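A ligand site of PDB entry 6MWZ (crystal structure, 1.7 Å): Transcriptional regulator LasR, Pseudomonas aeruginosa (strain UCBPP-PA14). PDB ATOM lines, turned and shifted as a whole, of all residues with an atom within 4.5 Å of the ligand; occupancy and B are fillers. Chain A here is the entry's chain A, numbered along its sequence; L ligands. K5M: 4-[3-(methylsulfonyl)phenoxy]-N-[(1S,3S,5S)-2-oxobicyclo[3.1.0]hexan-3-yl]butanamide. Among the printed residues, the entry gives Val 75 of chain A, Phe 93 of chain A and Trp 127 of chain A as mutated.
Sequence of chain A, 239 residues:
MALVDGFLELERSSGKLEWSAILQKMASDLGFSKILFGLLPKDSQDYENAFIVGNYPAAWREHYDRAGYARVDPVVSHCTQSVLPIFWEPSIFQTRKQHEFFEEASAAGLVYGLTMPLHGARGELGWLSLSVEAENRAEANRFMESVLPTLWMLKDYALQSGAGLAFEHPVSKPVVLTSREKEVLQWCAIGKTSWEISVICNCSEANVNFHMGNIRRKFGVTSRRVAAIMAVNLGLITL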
ATOM      1  N   LEU A  36      22.866  13.429  12.871  1.00  0.00           N
ATOM      2  CA  LEU A  36      21.868  14.201  13.584  1.00  0.00           C
ATOM      3  C   LEU A  36      22.414  14.452  14.981  1.00  0.00           C
ATOM      4  O   LEU A  36      22.707  13.497  15.702  1.00  0.00           O
ATOM      5  CB  LEU A  36      20.527  13.470  13.655  1.00  0.00           C
ATOM      6  CG  LEU A  36      19.323  14.279  14.137  1.00  0.00           C
ATOM      7  CD1 LEU A  36      18.950  15.334  13.123  1.00  0.00           C
ATOM      8  CD2 LEU A  36      18.165  13.329  14.353  1.00  0.00           C
ATOM      9  N   TYR A  47      10.485  17.152  21.988  1.00  0.00           N
ATOM     10  CA  TYR A  47      11.253  16.776  20.858  1.00  0.00           C
ATOM     11  C   TYR A  47      11.046  17.691  19.698  1.00  0.00           C
ATOM     12  O   TYR A  47      11.918  17.899  18.901  1.00  0.00           O
ATOM     13  CB  TYR A  47      10.939  15.401  20.400  1.00  0.00           C
ATOM     14  CG  TYR A  47      11.253  14.327  21.406  1.00  0.00           C
ATOM     15  CD1 TYR A  47      12.557  13.995  21.692  1.00  0.00           C
ATOM     16  CD2 TYR A  47      10.265  13.628  22.031  1.00  0.00           C
ATOM     17  CE1 TYR A  47      12.853  13.004  22.580  1.00  0.00           C
ATOM     18  CE2 TYR A  47      10.560  12.628  22.916  1.00  0.00           C
ATOM     19  CZ  TYR A  47      11.858  12.335  23.182  1.00  0.00           C
ATOM     20  OH  TYR A  47      12.177  11.353  24.073  1.00  0.00           O
ATOM     21  N   ILE A  52      18.461  20.962  16.880  1.00  0.00           N
ATOM     22  CA  ILE A  52      18.741  19.922  15.903  1.00  0.00           C
ATOM     23  C   ILE A  52      19.702  20.456  14.863  1.00  0.00           C
ATOM     24  O   ILE A  52      19.476  21.542  14.316  1.00  0.00           O
ATOM     25  CB  ILE A  52      17.446  19.411  15.238  1.00  0.00           C
ATOM     26  CG1 ILE A  52      16.489  18.807  16.263  1.00  0.00           C
ATOM     27  CG2 ILE A  52      17.780  18.387  14.150  1.00  0.00           C
ATOM     28  CD1 ILE A  52      16.834  17.401  16.667  1.00  0.00           C
ATOM     29  N   TYR A  56      20.400  14.742   8.300  1.00  0.00           N
ATOM     30  CA  TYR A  56      19.419  13.674   8.179  1.00  0.00           C
ATOM     31  C   TYR A  56      18.347  14.080   7.181  1.00  0.00           C
ATOM     32  O   TYR A  56      17.922  15.235   7.172  1.00  0.00           O
ATOM     33  CB  TYR A  56      18.717  13.397   9.519  1.00  0.00           C
ATOM     34  CG  TYR A  56      19.187  12.205  10.345  1.00  0.00           C
ATOM     35  CD1 TYR A  56      20.483  11.716  10.256  1.00  0.00           C
ATOM     36  CD2 TYR A  56      18.310  11.584  11.234  1.00  0.00           C
ATOM     37  CE1 TYR A  56      20.901  10.642  11.045  1.00  0.00           C
ATOM     38  CE2 TYR A  56      18.729  10.521  12.025  1.00  0.00           C
ATOM     39  CZ  TYR A  56      20.015  10.056  11.926  1.00  0.00           C
ATOM     40  OH  TYR A  56      20.432   8.990  12.694  1.00  0.00           O
ATOM     41  N   TRP A  60      12.644  11.878   6.438  1.00  0.00           N
ATOM     42  CA  TRP A  60      12.765  10.995   7.597  1.00  0.00           C
ATOM     43  C   TRP A  60      12.456  11.724   8.895  1.00  0.00           C
ATOM     44  O   TRP A  60      11.733  11.213   9.744  1.00  0.00           O
ATOM     45  CB  TRP A  60      14.166  10.385   7.647  1.00  0.00           C
ATOM     46  CG  TRP A  60      14.370   9.525   8.863  1.00  0.00           C
ATOM     47  CD1 TRP A  60      15.238   9.746   9.881  1.00  0.00           C
ATOM     48  CD2 TRP A  60      13.675   8.318   9.179  1.00  0.00           C
ATOM     49  NE1 TRP A  60      15.133   8.736  10.827  1.00  0.00           N
ATOM     50  CE2 TRP A  60      14.170   7.854  10.409  1.00  0.00           C
ATOM     51  CE3 TRP A  60      12.670   7.578   8.533  1.00  0.00           C
ATOM     52  CZ2 TRP A  60      13.710   6.687  11.013  1.00  0.00           C
ATOM     53  CZ3 TRP A  60      12.214   6.424   9.127  1.00  0.00           C
ATOM     54  CH2 TRP A  60      12.740   5.982  10.358  1.00  0.00           C
ATOM     55  N   ARG A  61      13.012  12.936   9.060  1.00  0.00           N
ATOM     56  CA  ARG A  61      12.777  13.663  10.302  1.00  0.00           C
ATOM     57  C   ARG A  61      11.290  13.952  10.482  1.00  0.00           C
ATOM     58  O   ARG A  61      10.747  13.818  11.584  1.00  0.00           O
ATOM     59  CB  ARG A  61      13.599  14.944  10.323  1.00  0.00           C
ATOM     60  CG  ARG A  61      15.094  14.707  10.241  1.00  0.00           C
ATOM     61  CD  ARG A  61      15.866  16.019  10.109  1.00  0.00           C
ATOM     62  NE  ARG A  61      15.481  16.967  11.140  1.00  0.00           N
ATOM     63  CZ  ARG A  61      15.021  18.200  10.937  1.00  0.00           C
ATOM     64  NH1 ARG A  61      14.893  18.652   9.707  1.00  0.00           N
ATOM     65  NH2 ARG A  61      14.693  18.950  11.988  1.00  0.00           N
ATOM     66  N   GLU A  62      10.596  14.301   9.400  1.00  0.00           N
ATOM     67  CA  GLU A  62       9.165  14.592   9.512  1.00  0.00           C
ATOM     68  C   GLU A  62       8.375  13.319   9.776  1.00  0.00           C
ATOM     69  O   GLU A  62       7.458  13.306  10.619  1.00  0.00           O
ATOM     70  CB  GLU A  62       8.688  15.300   8.246  1.00  0.00           C
ATOM     71  CG  GLU A  62       7.247  15.791   8.299  1.00  0.00           C
ATOM     72  CD  GLU A  62       6.998  16.747   9.460  1.00  0.00           C
ATOM     73  OE1 GLU A  62       7.905  17.537   9.806  1.00  0.00           O
ATOM     74  OE2 GLU A  62       5.887  16.701  10.030  1.00  0.00           O
ATOM     75  N   TYR A  64       9.492  10.628  11.245  1.00  0.00           N
ATOM     76  CA  TYR A  64       9.807  10.214  12.609  1.00  0.00           C
ATOM     77  C   TYR A  64       8.920  10.925  13.623  1.00  0.00           C
ATOM     78  O   TYR A  64       8.403  10.306  14.568  1.00  0.00           O
ATOM     79  CB  TYR A  64      11.282  10.515  12.868  1.00  0.00           C
ATOM     80  CG  TYR A  64      11.938   9.910  14.077  1.00  0.00           C
ATOM     81  CD1 TYR A  64      11.738  10.450  15.343  1.00  0.00           C
ATOM     82  CD2 TYR A  64      12.811   8.830  13.959  1.00  0.00           C
ATOM     83  CE1 TYR A  64      12.367   9.927  16.439  1.00  0.00           C
ATOM     84  CE2 TYR A  64      13.449   8.291  15.068  1.00  0.00           C
ATOM     85  CZ  TYR A  64      13.212   8.839  16.311  1.00  0.00           C
ATOM     86  OH  TYR A  64      13.829   8.328  17.430  1.00  0.00           O
ATOM     87  N   ASP A  73      11.843   3.912  18.822  1.00  0.00           N
ATOM     88  CA  ASP A  73      13.231   3.759  18.432  1.00  0.00           C
ATOM     89  C   ASP A  73      14.052   3.258  19.617  1.00  0.00           C
ATOM     90  O   ASP A  73      14.131   3.963  20.645  1.00  0.00           O
ATOM     91  CB  ASP A  73      13.707   5.119  17.946  1.00  0.00           C
ATOM     92  CG  ASP A  73      15.163   5.132  17.502  1.00  0.00           C
ATOM     93  OD1 ASP A  73      15.843   4.095  17.535  1.00  0.00           O
ATOM     94  OD2 ASP A  73      15.562   6.220  17.039  1.00  0.00           O
ATOM     95  N   VAL A  75      17.115   3.264  20.022  1.00  0.00           N
ATOM     96  CA  VAL A  75      18.234   4.160  20.305  1.00  0.00           C
ATOM     97  C   VAL A  75      17.835   5.211  21.343  1.00  0.00           C
ATOM     98  O   VAL A  75      18.630   5.548  22.239  1.00  0.00           O
ATOM     99  CB  VAL A  75      18.746   4.831  19.019  1.00  0.00           C
ATOM    100  CG1 VAL A  75      19.794   5.911  19.382  1.00  0.00           C
ATOM    101  CG2 VAL A  75      19.342   3.785  18.121  1.00  0.00           C
ATOM    102  N   VAL A  76      16.604   5.717  21.256  1.00  0.00           N
ATOM    103  CA  VAL A  76      16.183   6.771  22.163  1.00  0.00           C
ATOM    104  C   VAL A  76      16.059   6.232  23.583  1.00  0.00           C
ATOM    105  O   VAL A  76      16.557   6.849  24.530  1.00  0.00           O
ATOM    106  CB  VAL A  76      14.872   7.409  21.661  1.00  0.00           C
ATOM    107  CG1 VAL A  76      14.283   8.343  22.733  1.00  0.00           C
ATOM    108  CG2 VAL A  76      15.140   8.191  20.361  1.00  0.00           C
ATOM    109  N   TRP A  88      23.712   0.546  15.373  1.00  0.00           N
ATOM    110  CA  TRP A  88      22.401   0.221  14.782  1.00  0.00           C
ATOM    111  C   TRP A  88      22.367  -1.231  14.268  1.00  0.00           C
ATOM    112  O   TRP A  88      22.142  -1.503  13.087  1.00  0.00           O
ATOM    113  CB  TRP A  88      22.047   1.184  13.665  1.00  0.00           C
ATOM    114  CG  TRP A  88      22.040   2.626  14.054  1.00  0.00           C
ATOM    115  CD1 TRP A  88      22.059   3.145  15.319  1.00  0.00           C
ATOM    116  CD2 TRP A  88      22.038   3.736  13.157  1.00  0.00           C
ATOM    117  NE1 TRP A  88      22.076   4.531  15.253  1.00  0.00           N
ATOM    118  CE2 TRP A  88      22.067   4.906  13.939  1.00  0.00           C
ATOM    119  CE3 TRP A  88      22.020   3.855  11.760  1.00  0.00           C
ATOM    120  CZ2 TRP A  88      22.053   6.192  13.363  1.00  0.00           C
ATOM    121  CZ3 TRP A  88      22.024   5.127  11.193  1.00  0.00           C
ATOM    122  CH2 TRP A  88      22.045   6.269  11.994  1.00  0.00           C
ATOM    123  N   PHE A  93      16.503  -3.997  17.058  1.00  0.00           N
ATOM    124  CA  PHE A  93      15.152  -3.734  16.570  1.00  0.00           C
ATOM    125  C   PHE A  93      14.377  -5.041  16.718  1.00  0.00           C
ATOM    126  O   PHE A  93      14.312  -5.871  15.808  1.00  0.00           O
ATOM    127  CB  PHE A  93      15.191  -3.220  15.131  1.00  0.00           C
ATOM    128  CG  PHE A  93      16.087  -2.021  14.960  1.00  0.00           C
ATOM    129  CD1 PHE A  93      15.654  -0.774  15.362  1.00  0.00           C
ATOM    130  CD2 PHE A  93      17.358  -2.161  14.438  1.00  0.00           C
ATOM    131  CE1 PHE A  93      16.472   0.338  15.230  1.00  0.00           C
ATOM    132  CE2 PHE A  93      18.182  -1.062  14.311  1.00  0.00           C
ATOM    133  CZ  PHE A  93      17.743   0.188  14.705  1.00  0.00           C
ATOM    134  N   PHE A 101      10.070   0.079  11.989  1.00  0.00           N
ATOM    135  CA  PHE A 101      10.793   1.341  12.097  1.00  0.00           C
ATOM    136  C   PHE A 101      12.121   1.282  11.340  1.00  0.00           C
ATOM    137  O   PHE A 101      12.472   2.192  10.592  1.00  0.00           O
ATOM    138  CB  PHE A 101      10.992   1.660  13.574  1.00  0.00           C
ATOM    139  CG  PHE A 101      12.074   2.656  13.842  1.00  0.00           C
ATOM    140  CD1 PHE A 101      11.818   4.004  13.765  1.00  0.00           C
ATOM    141  CD2 PHE A 101      13.358   2.227  14.166  1.00  0.00           C
ATOM    142  CE1 PHE A 101      12.836   4.937  13.999  1.00  0.00           C
ATOM    143  CE2 PHE A 101      14.367   3.159  14.405  1.00  0.00           C
ATOM    144  CZ  PHE A 101      14.106   4.500  14.316  1.00  0.00           C
ATOM    145  N   PHE A 102      12.875   0.185  11.516  1.00  0.00           N
ATOM    146  CA  PHE A 102      14.176   0.125  10.883  1.00  0.00           C
ATOM    147  C   PHE A 102      14.042  -0.093   9.390  1.00  0.00           C
ATOM    148  O   PHE A 102      14.903   0.344   8.605  1.00  0.00           O
ATOM    149  CB  PHE A 102      15.019  -0.969  11.514  1.00  0.00           C
ATOM    150  CG  PHE A 102      16.490  -0.815  11.278  1.00  0.00           C
ATOM    151  CD1 PHE A 102      17.084   0.426  11.418  1.00  0.00           C
ATOM    152  CD2 PHE A 102      17.268  -1.894  10.938  1.00  0.00           C
ATOM    153  CE1 PHE A 102      18.453   0.581  11.206  1.00  0.00           C
ATOM    154  CE2 PHE A 102      18.642  -1.751  10.731  1.00  0.00           C
ATOM    155  CZ  PHE A 102      19.232  -0.507  10.863  1.00  0.00           C
ATOM    156  N   ALA A 105      13.588   3.324   8.146  1.00  0.00           N
ATOM    157  CA  ALA A 105      14.841   3.999   8.240  1.00  0.00           C
ATOM    158  C   ALA A 105      15.695   3.672   7.028  1.00  0.00           C
ATOM    159  O   ALA A 105      16.313   4.512   6.486  1.00  0.00           O
ATOM    160  CB  ALA A 105      15.569   3.617   9.507  1.00  0.00           C
ATOM    161  N   LEU A 110      19.221   5.198   6.079  1.00  0.00           N
ATOM    162  CA  LEU A 110      19.890   5.059   7.380  1.00  0.00           C
ATOM    163  C   LEU A 110      19.970   3.576   7.730  1.00  0.00           C
ATOM    164  O   LEU A 110      19.093   3.039   8.406  1.00  0.00           O
ATOM    165  CB  LEU A 110      19.146   5.861   8.437  1.00  0.00           C
ATOM    166  CG  LEU A 110      19.091   7.370   8.165  1.00  0.00           C
ATOM    167  CD1 LEU A 110      18.152   8.053   9.138  1.00  0.00           C
ATOM    168  CD2 LEU A 110      20.487   7.984   8.251  1.00  0.00           C
ATOM    169  N   THR A 115      24.853   5.666  17.550  1.00  0.00           N
ATOM    170  CA  THR A 115      24.458   6.866  18.275  1.00  0.00           C
ATOM    171  C   THR A 115      25.245   6.969  19.578  1.00  0.00           C
ATOM    172  O   THR A 115      25.355   5.979  20.309  1.00  0.00           O
ATOM    173  CB  THR A 115      22.946   6.875  18.531  1.00  0.00           C
ATOM    174  OG1 THR A 115      22.264   6.831  17.271  1.00  0.00           O
ATOM    175  CG2 THR A 115      22.525   8.154  19.274  1.00  0.00           C
ATOM    176  N   TRP A 127      21.601  13.321  21.690  1.00  0.00           N
ATOM    177  CA  TRP A 127      22.213  12.228  20.960  1.00  0.00           C
ATOM    178  C   TRP A 127      23.051  12.807  19.850  1.00  0.00           C
ATOM    179  O   TRP A 127      22.749  13.872  19.305  1.00  0.00           O
ATOM    180  CB  TRP A 127      21.158  11.287  20.346  1.00  0.00           C
ATOM    181  CG  TRP A 127      19.999  12.034  19.864  1.00  0.00           C
ATOM    182  CD1 TRP A 127      19.866  12.696  18.672  1.00  0.00           C
ATOM    183  CD2 TRP A 127      18.779  12.275  20.584  1.00  0.00           C
ATOM    184  NE1 TRP A 127      18.648  13.312  18.603  1.00  0.00           N
ATOM    185  CE2 TRP A 127      17.960  13.074  19.766  1.00  0.00           C
ATOM    186  CE3 TRP A 127      18.303  11.870  21.833  1.00  0.00           C
ATOM    187  CZ2 TRP A 127      16.681  13.478  20.165  1.00  0.00           C
ATOM    188  CZ3 TRP A 127      17.046  12.274  22.231  1.00  0.00           C
ATOM    189  CH2 TRP A 127      16.245  13.066  21.400  1.00  0.00           C
ATOM    190  N   SER A 129      23.954  11.049  16.430  1.00  0.00           N
ATOM    191  CA  SER A 129      23.792   9.892  15.549  1.00  0.00           C
ATOM    192  C   SER A 129      24.574  10.114  14.277  1.00  0.00           C
ATOM    193  O   SER A 129      24.548  11.200  13.699  1.00  0.00           O
ATOM    194  CB  SER A 129      22.314   9.676  15.225  1.00  0.00           C
ATOM    195  OG  SER A 129      21.660   9.106  16.339  1.00  0.00           O
HETATM  196  C10 K5M L   1      14.557  12.678  16.977  1.00  0.00           C
HETATM  197  C13 K5M L   1      12.429  14.353  16.134  1.00  0.00           C
HETATM  198  C21 K5M L   1      17.887   4.553  14.428  1.00  0.00           C
HETATM  199  C22 K5M L   1      17.737   4.227  13.064  1.00  0.00           C
HETATM  200  C24 K5M L   1      18.567   4.416  11.765  1.00  0.00           C
HETATM  201  C02 K5M L   1      17.471   6.657  13.315  1.00  0.00           C
HETATM  202  C03 K5M L   1      18.203   6.188  14.406  1.00  0.00           C
HETATM  203  C05 K5M L   1      18.385   8.191  15.964  1.00  0.00           C
HETATM  204  C06 K5M L   1      17.873   8.933  17.227  1.00  0.00           C
HETATM  205  C07 K5M L   1      17.573  10.439  16.965  1.00  0.00           C
HETATM  206  C08 K5M L   1      16.145  10.856  16.491  1.00  0.00           C
HETATM  207  C11 K5M L   1      13.320  12.682  17.649  1.00  0.00           C
HETATM  208  C12 K5M L   1      12.256  13.505  17.223  1.00  0.00           C
HETATM  209  C14 K5M L   1      13.657  14.357  15.470  1.00  0.00           C
HETATM  210  C16 K5M L   1      15.627  15.093  13.345  1.00  0.00           C
HETATM  211  C19 K5M L   1      14.707  13.536  15.892  1.00  0.00           C
HETATM  212  C23 K5M L   1      17.550   5.515  12.202  1.00  0.00           C
HETATM  213  N04 K5M L   1      17.797   6.884  15.617  1.00  0.00           N
HETATM  214  O01 K5M L   1      16.856   7.648  13.107  1.00  0.00           O
HETATM  215  O09 K5M L   1      15.647  11.850  17.386  1.00  0.00           O
HETATM  216  O17 K5M L   1      12.918  15.370  13.037  1.00  0.00           O
HETATM  217  O18 K5M L   1      13.912  16.847  14.461  1.00  0.00           O
HETATM  218  O20 K5M L   1      19.221   8.685  15.260  1.00  0.00           O
HETATM  219  S15 K5M L   1      13.975  15.448  14.041  1.00  0.00           S
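O20 of the ligand lies within hydrogen-bond range of OG of Ser 129 (2.7 Å).
NH2 of Arg 61 is in hydrogen-bond range of O18 of the ligand (3.3 Å).
The indole nitrogen of Trp 60 sits at hydrogen-bond distance from an oxygen (O01) of the ligand.
The side-chain hydroxyl of Tyr 56 sits at hydrogen-bond distance from an oxygen (O20) of the ligand, 2.9 Å away.
A nitrogen (N04) of the ligand lies within hydrogen-bond range of the side-chain carboxylate (OD2) of Asp 73, 2.7 Å away.
The backbone carbonyl oxygen (O) of Leu 36 sits at hydrogen-bond distance from the backbone NH (N) of Ser 129 (2.8 Å).
The backbone NH (N) of Val 75 lies within hydrogen-bond range of the side-chain carboxylate (OD1) of Asp 73 (2.9 Å).
The indole nitrogen (NE1) of Trp 88 lies within hydrogen-bond range of the side-chain hydroxyl (OG1) of Thr 115, at 3.1 Å.
The side-chain carboxylate (OD2) of Asp 73 is in hydrogen-bond range of the side-chain hydroxyl (OH) of Tyr 64 (2.8 Å).
N of Leu 110 is in hydrogen-bond range of O of Ala 105 (3.0 Å).
The side-chain hydroxyl (OG) of Ser 129 sits at hydrogen-bond distance from the side-chain hydroxyl (OG1) of Thr 115 (2.5 Å).
CD2 of Leu 36 touches C16 of the ligand, 3.3 Å away.
CB of Tyr 47 touches C12 of the ligand, at 3.9 Å.
CD1 of Ile 52 touches O18 of the ligand, 3.7 Å away.
CE1 of Tyr 64 touches C11 of the ligand (3.2 Å).
Trp 88 touches the ligand.
Phe 101 touches the ligand (CE2 to C22, 3.8 Å).
Phe 102 touches the ligand.
CB of Ala 105 touches C24 of the ligand, at 3.8 Å.
O of Leu 110 touches C24 of the ligand, 3.7 Å away.
CZ2 of Trp 127 touches O09 of the ligand, 3.4 Å away.
Of the 20 residues printed, 15 come within 4 Å of the ligand.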
